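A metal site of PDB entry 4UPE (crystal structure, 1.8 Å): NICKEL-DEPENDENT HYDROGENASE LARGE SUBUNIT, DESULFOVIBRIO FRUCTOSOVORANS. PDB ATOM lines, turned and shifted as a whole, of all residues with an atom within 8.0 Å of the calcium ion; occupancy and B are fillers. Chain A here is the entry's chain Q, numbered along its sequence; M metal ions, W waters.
ND1 of His 548 lies close to O of Gly 546. OE1 of Glu 52 lies within hydrogen-bond range of OG1 of Thr 354, 2.7 Å away. The side-chain amide oxygen of Gln 493 sits close to the side-chain carboxylate of Glu 52. ND1 of His 548 lies within hydrogen-bond range of O of Cys 545 (2.7 Å).
The calcium ion is bound by water W1 (2.1 Å), water W2 (2.2 Å), the backbone carbonyl oxygen (O) of Leu 494 (2.2 Å), water W3 (2.2 Å), a ring nitrogen (NE2) of His 548 (2.3 Å) and the side-chain carboxylate (OE2) of Glu 52 (2.3 Å).
Water W2 lies within hydrogen-bond range of the side-chain carboxylate (OE1) of Glu 333, the side-chain amide oxygen (OE1) of Gln 493 and the side-chain amino group (NZ) of Lys 371. Water W3 bridges the side-chain carboxylate (OE1) of Glu 52 (2.7 Å) and the side-chain amino group (NZ) of Lys 371 (3.1 Å).
Three residues have an atom within 4 Å of the calcium ion: Glu 52, Leu 494 and His 548. Along chain A the residues within 4 Å of the calcium ion span positions 52 to 548.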
ATOM      1  N   GLU A  52      -2.711  24.226  19.503  1.00  0.00           N
ATOM      2  CA  GLU A  52      -4.117  24.567  19.572  1.00  0.00           C
ATOM      3  C   GLU A  52      -4.449  25.311  20.858  1.00  0.00           C
ATOM      4  O   GLU A  52      -5.284  26.199  20.850  1.00  0.00           O
ATOM      5  CB  GLU A  52      -4.977  23.306  19.438  1.00  0.00           C
ATOM      6  CG  GLU A  52      -4.688  22.547  18.149  1.00  0.00           C
ATOM      7  CD  GLU A  52      -5.116  21.081  18.213  1.00  0.00           C
ATOM      8  OE1 GLU A  52      -5.004  20.422  19.300  1.00  0.00           O
ATOM      9  OE2 GLU A  52      -5.481  20.567  17.145  1.00  0.00           O
ATOM     10  N   GLU A 333     -12.445  12.992  16.250  1.00  0.00           N
ATOM     11  CA  GLU A 333     -11.224  12.430  16.836  1.00  0.00           C
ATOM     12  C   GLU A 333     -11.489  11.797  18.190  1.00  0.00           C
ATOM     13  O   GLU A 333     -12.243  12.372  19.016  1.00  0.00           O
ATOM     14  CB  GLU A 333     -10.159  13.513  16.988  1.00  0.00           C
ATOM     15  CG  GLU A 333      -9.670  14.078  15.657  1.00  0.00           C
ATOM     16  CD  GLU A 333      -8.668  15.209  15.839  1.00  0.00           C
ATOM     17  OE1 GLU A 333      -9.048  16.300  16.354  1.00  0.00           O
ATOM     18  OE2 GLU A 333      -7.468  14.991  15.485  1.00  0.00           O
ATOM     19  N   TYR A 340      -4.532  12.199  26.682  1.00  0.00           N
ATOM     20  CA  TYR A 340      -5.470  13.310  26.948  1.00  0.00           C
ATOM     21  C   TYR A 340      -6.416  12.883  28.023  1.00  0.00           C
ATOM     22  O   TYR A 340      -6.565  11.696  28.269  1.00  0.00           O
ATOM     23  CB  TYR A 340      -6.197  13.762  25.650  1.00  0.00           C
ATOM     24  CG  TYR A 340      -5.200  14.285  24.636  1.00  0.00           C
ATOM     25  CD1 TYR A 340      -4.653  15.580  24.749  1.00  0.00           C
ATOM     26  CD2 TYR A 340      -4.726  13.462  23.612  1.00  0.00           C
ATOM     27  CE1 TYR A 340      -3.684  16.040  23.846  1.00  0.00           C
ATOM     28  CE2 TYR A 340      -3.766  13.900  22.717  1.00  0.00           C
ATOM     29  CZ  TYR A 340      -3.234  15.182  22.840  1.00  0.00           C
ATOM     30  OH  TYR A 340      -2.277  15.580  21.915  1.00  0.00           O
ATOM     31  N   PRO A 349     -14.024  18.265  14.839  1.00  0.00           N
ATOM     32  CA  PRO A 349     -13.030  19.307  15.137  1.00  0.00           C
ATOM     33  C   PRO A 349     -13.548  20.692  15.511  1.00  0.00           C
ATOM     34  O   PRO A 349     -12.838  21.421  16.194  1.00  0.00           O
ATOM     35  CB  PRO A 349     -12.182  19.355  13.852  1.00  0.00           C
ATOM     36  CG  PRO A 349     -12.273  17.956  13.325  1.00  0.00           C
ATOM     37  CD  PRO A 349     -13.698  17.546  13.605  1.00  0.00           C
ATOM     38  N   GLY A 352     -13.484  20.428  19.037  1.00  0.00           N
ATOM     39  CA  GLY A 352     -12.270  19.740  19.459  1.00  0.00           C
ATOM     40  C   GLY A 352     -11.851  20.155  20.855  1.00  0.00           C
ATOM     41  O   GLY A 352     -12.087  21.303  21.239  1.00  0.00           O
ATOM     42  N   VAL A 353     -11.295  19.219  21.623  1.00  0.00           N
ATOM     43  CA  VAL A 353     -10.771  19.486  22.963  1.00  0.00           C
ATOM     44  C   VAL A 353      -9.318  18.979  23.007  1.00  0.00           C
ATOM     45  O   VAL A 353      -9.043  17.902  22.508  1.00  0.00           O
ATOM     46  CB  VAL A 353     -11.639  18.768  24.041  1.00  0.00           C
ATOM     47  CG1 VAL A 353     -10.963  18.789  25.420  1.00  0.00           C
ATOM     48  CG2 VAL A 353     -13.020  19.401  24.139  1.00  0.00           C
ATOM     49  N   THR A 354      -8.402  19.763  23.596  1.00  0.00           N
ATOM     50  CA  THR A 354      -6.983  19.366  23.688  1.00  0.00           C
ATOM     51  C   THR A 354      -6.557  19.547  25.145  1.00  0.00           C
ATOM     52  O   THR A 354      -6.097  20.620  25.545  1.00  0.00           O
ATOM     53  CB  THR A 354      -6.125  20.135  22.653  1.00  0.00           C
ATOM     54  OG1 THR A 354      -6.703  19.943  21.353  1.00  0.00           O
ATOM     55  CG2 THR A 354      -4.634  19.673  22.615  1.00  0.00           C
ATOM     56  N   TRP A 369       0.768  10.774  22.075  1.00  0.00           N
ATOM     57  CA  TRP A 369       0.363  12.185  22.042  1.00  0.00           C
ATOM     58  C   TRP A 369      -0.525  12.558  20.840  1.00  0.00           C
ATOM     59  O   TRP A 369      -1.152  13.626  20.837  1.00  0.00           O
ATOM     60  CB  TRP A 369       1.594  13.082  22.048  1.00  0.00           C
ATOM     61  CG  TRP A 369       2.201  13.156  23.407  1.00  0.00           C
ATOM     62  CD1 TRP A 369       3.417  12.679  23.806  1.00  0.00           C
ATOM     63  CD2 TRP A 369       1.608  13.765  24.555  1.00  0.00           C
ATOM     64  NE1 TRP A 369       3.620  12.944  25.137  1.00  0.00           N
ATOM     65  CE2 TRP A 369       2.507  13.586  25.636  1.00  0.00           C
ATOM     66  CE3 TRP A 369       0.371  14.416  24.804  1.00  0.00           C
ATOM     67  CZ2 TRP A 369       2.248  14.080  26.913  1.00  0.00           C
ATOM     68  CZ3 TRP A 369       0.106  14.889  26.063  1.00  0.00           C
ATOM     69  CH2 TRP A 369       1.048  14.726  27.110  1.00  0.00           C
ATOM     70  N   MET A 370      -0.599  11.676  19.838  1.00  0.00           N
ATOM     71  CA  MET A 370      -1.614  11.832  18.755  1.00  0.00           C
ATOM     72  C   MET A 370      -3.008  11.446  19.181  1.00  0.00           C
ATOM     73  O   MET A 370      -3.204  10.463  19.929  1.00  0.00           O
ATOM     74  CB  MET A 370      -1.235  10.985  17.547  1.00  0.00           C
ATOM     75  CG  MET A 370      -0.019  11.529  16.794  1.00  0.00           C
ATOM     76  SD  MET A 370       0.007  10.915  15.106  1.00  0.00           S
ATOM     77  CE  MET A 370       1.740  11.194  14.739  1.00  0.00           C
ATOM     78  N   LYS A 371      -3.984  12.236  18.725  1.00  0.00           N
ATOM     79  CA  LYS A 371      -5.372  11.829  18.780  1.00  0.00           C
ATOM     80  C   LYS A 371      -5.590  10.777  17.691  1.00  0.00           C
ATOM     81  O   LYS A 371      -4.715  10.539  16.877  1.00  0.00           O
ATOM     82  CB  LYS A 371      -6.319  13.027  18.601  1.00  0.00           C
ATOM     83  CG  LYS A 371      -6.143  14.141  19.625  1.00  0.00           C
ATOM     84  CD  LYS A 371      -7.175  15.231  19.426  1.00  0.00           C
ATOM     85  CE  LYS A 371      -6.976  16.356  20.428  1.00  0.00           C
ATOM     86  NZ  LYS A 371      -7.781  17.549  20.024  1.00  0.00           N
ATOM     87  N   PRO A 373      -8.013  10.177  14.713  1.00  0.00           N
ATOM     88  CA  PRO A 373      -9.114  10.572  13.833  1.00  0.00           C
ATOM     89  C   PRO A 373      -9.810   9.358  13.224  1.00  0.00           C
ATOM     90  O   PRO A 373      -9.161   8.417  12.733  1.00  0.00           O
ATOM     91  CB  PRO A 373      -8.419  11.387  12.735  1.00  0.00           C
ATOM     92  CG  PRO A 373      -7.016  11.675  13.245  1.00  0.00           C
ATOM     93  CD  PRO A 373      -6.710  10.476  14.113  1.00  0.00           C
ATOM     94  N   SER A 479      -6.739  19.285   7.497  1.00  0.00           N
ATOM     95  CA  SER A 479      -7.857  20.225   7.749  1.00  0.00           C
ATOM     96  C   SER A 479      -7.661  21.054   9.010  1.00  0.00           C
ATOM     97  O   SER A 479      -7.231  20.521  10.101  1.00  0.00           O
ATOM     98  CB  SER A 479      -9.204  19.470   7.764  1.00  0.00           C
ATOM     99  OG  SER A 479      -9.211  18.482   8.795  1.00  0.00           O
ATOM    100  N   TRP A 481      -9.634  23.966  11.520  1.00  0.00           N
ATOM    101  CA  TRP A 481     -11.017  24.322  11.864  1.00  0.00           C
ATOM    102  C   TRP A 481     -11.006  25.417  12.920  1.00  0.00           C
ATOM    103  O   TRP A 481     -10.429  25.237  13.993  1.00  0.00           O
ATOM    104  CB  TRP A 481     -11.770  23.067  12.409  1.00  0.00           C
ATOM    105  CG  TRP A 481     -11.588  21.787  11.617  1.00  0.00           C
ATOM    106  CD1 TRP A 481     -10.435  21.005  11.526  1.00  0.00           C
ATOM    107  CD2 TRP A 481     -12.573  21.131  10.816  1.00  0.00           C
ATOM    108  NE1 TRP A 481     -10.668  19.915  10.724  1.00  0.00           N
ATOM    109  CE2 TRP A 481     -11.967  19.975  10.263  1.00  0.00           C
ATOM    110  CE3 TRP A 481     -13.901  21.438  10.472  1.00  0.00           C
ATOM    111  CZ2 TRP A 481     -12.658  19.105   9.404  1.00  0.00           C
ATOM    112  CZ3 TRP A 481     -14.589  20.580   9.621  1.00  0.00           C
ATOM    113  CH2 TRP A 481     -13.963  19.426   9.091  1.00  0.00           C
ATOM    114  N   PHE A 492      -9.343  26.473  17.807  1.00  0.00           N
ATOM    115  CA  PHE A 492      -8.657  26.217  16.554  1.00  0.00           C
ATOM    116  C   PHE A 492      -8.091  24.828  16.634  1.00  0.00           C
ATOM    117  O   PHE A 492      -7.272  24.572  17.501  1.00  0.00           O
ATOM    118  CB  PHE A 492      -7.492  27.212  16.342  1.00  0.00           C
ATOM    119  CG  PHE A 492      -7.098  27.349  14.898  1.00  0.00           C
ATOM    120  CD1 PHE A 492      -6.310  26.374  14.276  1.00  0.00           C
ATOM    121  CD2 PHE A 492      -7.536  28.437  14.156  1.00  0.00           C
ATOM    122  CE1 PHE A 492      -5.983  26.495  12.921  1.00  0.00           C
ATOM    123  CE2 PHE A 492      -7.206  28.569  12.809  1.00  0.00           C
ATOM    124  CZ  PHE A 492      -6.419  27.594  12.187  1.00  0.00           C
ATOM    125  N   GLN A 493      -8.549  23.939  15.757  1.00  0.00           N
ATOM    126  CA  GLN A 493      -8.159  22.543  15.822  1.00  0.00           C
ATOM    127  C   GLN A 493      -7.514  22.157  14.514  1.00  0.00           C
ATOM    128  O   GLN A 493      -8.011  22.542  13.435  1.00  0.00           O
ATOM    129  CB  GLN A 493      -9.376  21.669  16.119  1.00  0.00           C
ATOM    130  CG  GLN A 493      -9.989  21.891  17.508  1.00  0.00           C
ATOM    131  CD  GLN A 493      -9.116  21.300  18.607  1.00  0.00           C
ATOM    132  OE1 GLN A 493      -8.515  20.232  18.445  1.00  0.00           O
ATOM    133  NE2 GLN A 493      -9.010  22.015  19.727  1.00  0.00           N
ATOM    134  N   LEU A 494      -6.396  21.442  14.607  1.00  0.00           N
ATOM    135  CA  LEU A 494      -5.715  20.882  13.414  1.00  0.00           C
ATOM    136  C   LEU A 494      -5.990  19.398  13.391  1.00  0.00           C
ATOM    137  O   LEU A 494      -5.888  18.751  14.431  1.00  0.00           O
ATOM    138  CB  LEU A 494      -4.194  21.096  13.490  1.00  0.00           C
ATOM    139  CG  LEU A 494      -3.605  22.517  13.360  1.00  0.00           C
ATOM    140  CD1 LEU A 494      -3.979  23.413  14.514  1.00  0.00           C
ATOM    141  CD2 LEU A 494      -2.073  22.471  13.225  1.00  0.00           C
ATOM    142  N   VAL A 495      -6.376  18.848  12.225  1.00  0.00           N
ATOM    143  CA  VAL A 495      -6.431  17.393  12.047  1.00  0.00           C
ATOM    144  C   VAL A 495      -5.528  17.120  10.836  1.00  0.00           C
ATOM    145  O   VAL A 495      -5.797  17.586   9.730  1.00  0.00           O
ATOM    146  CB  VAL A 495      -7.856  16.833  11.829  1.00  0.00           C
ATOM    147  CG1 VAL A 495      -7.872  15.293  11.827  1.00  0.00           C
ATOM    148  CG2 VAL A 495      -8.850  17.409  12.860  1.00  0.00           C
ATOM    149  N   VAL A 496      -4.464  16.362  11.069  1.00  0.00           N
ATOM    150  CA  VAL A 496      -3.300  16.431  10.202  1.00  0.00           C
ATOM    151  C   VAL A 496      -3.116  15.030   9.585  1.00  0.00           C
ATOM    152  O   VAL A 496      -3.573  14.038  10.165  1.00  0.00           O
ATOM    153  CB  VAL A 496      -2.070  16.975  10.980  1.00  0.00           C
ATOM    154  CG1 VAL A 496      -0.865  17.239  10.096  1.00  0.00           C
ATOM    155  CG2 VAL A 496      -2.463  18.285  11.677  1.00  0.00           C
ATOM    156  N   THR A 499      -1.794  12.417  11.731  1.00  0.00           N
ATOM    157  CA  THR A 499      -2.726  12.066  12.762  1.00  0.00           C
ATOM    158  C   THR A 499      -3.617  10.928  12.251  1.00  0.00           C
ATOM    159  O   THR A 499      -3.840   9.993  12.995  1.00  0.00           O
ATOM    160  CB  THR A 499      -3.633  13.249  13.243  1.00  0.00           C
ATOM    161  OG1 THR A 499      -2.907  14.481  13.236  1.00  0.00           O
ATOM    162  CG2 THR A 499      -4.121  12.970  14.641  1.00  0.00           C
ATOM    163  N   CYS A 545       3.832  17.286  12.860  1.00  0.00           N
ATOM    164  CA  CYS A 545       2.505  17.453  12.215  1.00  0.00           C
ATOM    165  C   CYS A 545       1.407  16.665  12.981  1.00  0.00           C
ATOM    166  O   CYS A 545       0.381  17.229  13.376  1.00  0.00           O
ATOM    167  CB  CYS A 545       2.524  16.922  10.773  1.00  0.00           C
ATOM    168  SG  CYS A 545       2.848  18.205   9.578  1.00  0.00           S
ATOM    169  N   GLY A 546       1.638  15.373  13.189  1.00  0.00           N
ATOM    170  CA  GLY A 546       0.652  14.468  13.833  1.00  0.00           C
ATOM    171  C   GLY A 546       0.128  15.006  15.142  1.00  0.00           C
ATOM    172  O   GLY A 546      -1.089  14.963  15.401  1.00  0.00           O
ATOM    173  N   VAL A 547       1.028  15.500  15.989  1.00  0.00           N
ATOM    174  CA  VAL A 547       0.656  15.889  17.376  1.00  0.00           C
ATOM    175  C   VAL A 547       0.350  17.385  17.506  1.00  0.00           C
ATOM    176  O   VAL A 547      -0.604  17.778  18.186  1.00  0.00           O
ATOM    177  CB  VAL A 547       1.759  15.529  18.422  1.00  0.00           C
ATOM    178  CG1 VAL A 547       1.322  16.037  19.786  1.00  0.00           C
ATOM    179  CG2 VAL A 547       2.003  14.021  18.502  1.00  0.00           C
ATOM    180  N   HIS A 548       1.187  18.204  16.868  1.00  0.00           N
ATOM    181  CA  HIS A 548       1.119  19.672  16.977  1.00  0.00           C
ATOM    182  C   HIS A 548       0.960  20.144  18.435  1.00  0.00           C
ATOM    183  O   HIS A 548       0.147  21.021  18.736  1.00  0.00           O
ATOM    184  CB  HIS A 548       0.071  20.312  15.979  1.00  0.00           C
ATOM    185  CG  HIS A 548      -1.220  19.554  15.875  1.00  0.00           C
ATOM    186  ND1 HIS A 548      -1.349  18.423  15.091  1.00  0.00           N
ATOM    187  CD2 HIS A 548      -2.409  19.717  16.505  1.00  0.00           C
ATOM    188  CE1 HIS A 548      -2.572  17.924  15.230  1.00  0.00           C
ATOM    189  NE2 HIS A 548      -3.240  18.707  16.080  1.00  0.00           N
ATOM    190  OXT HIS A 548       1.666  19.651  19.337  1.00  0.00           O
HETATM  191 CA    CA M   1      -5.459  18.343  16.541  1.00  0.00          CA
HETATM  192  O   HOH W   1      -5.226  16.311  16.042  1.00  0.00           O
HETATM  193  O   HOH W   2      -7.547  18.144  17.016  1.00  0.00           O
HETATM  194  O   HOH W   3      -4.963  17.791  18.646  1.00  0.00           O
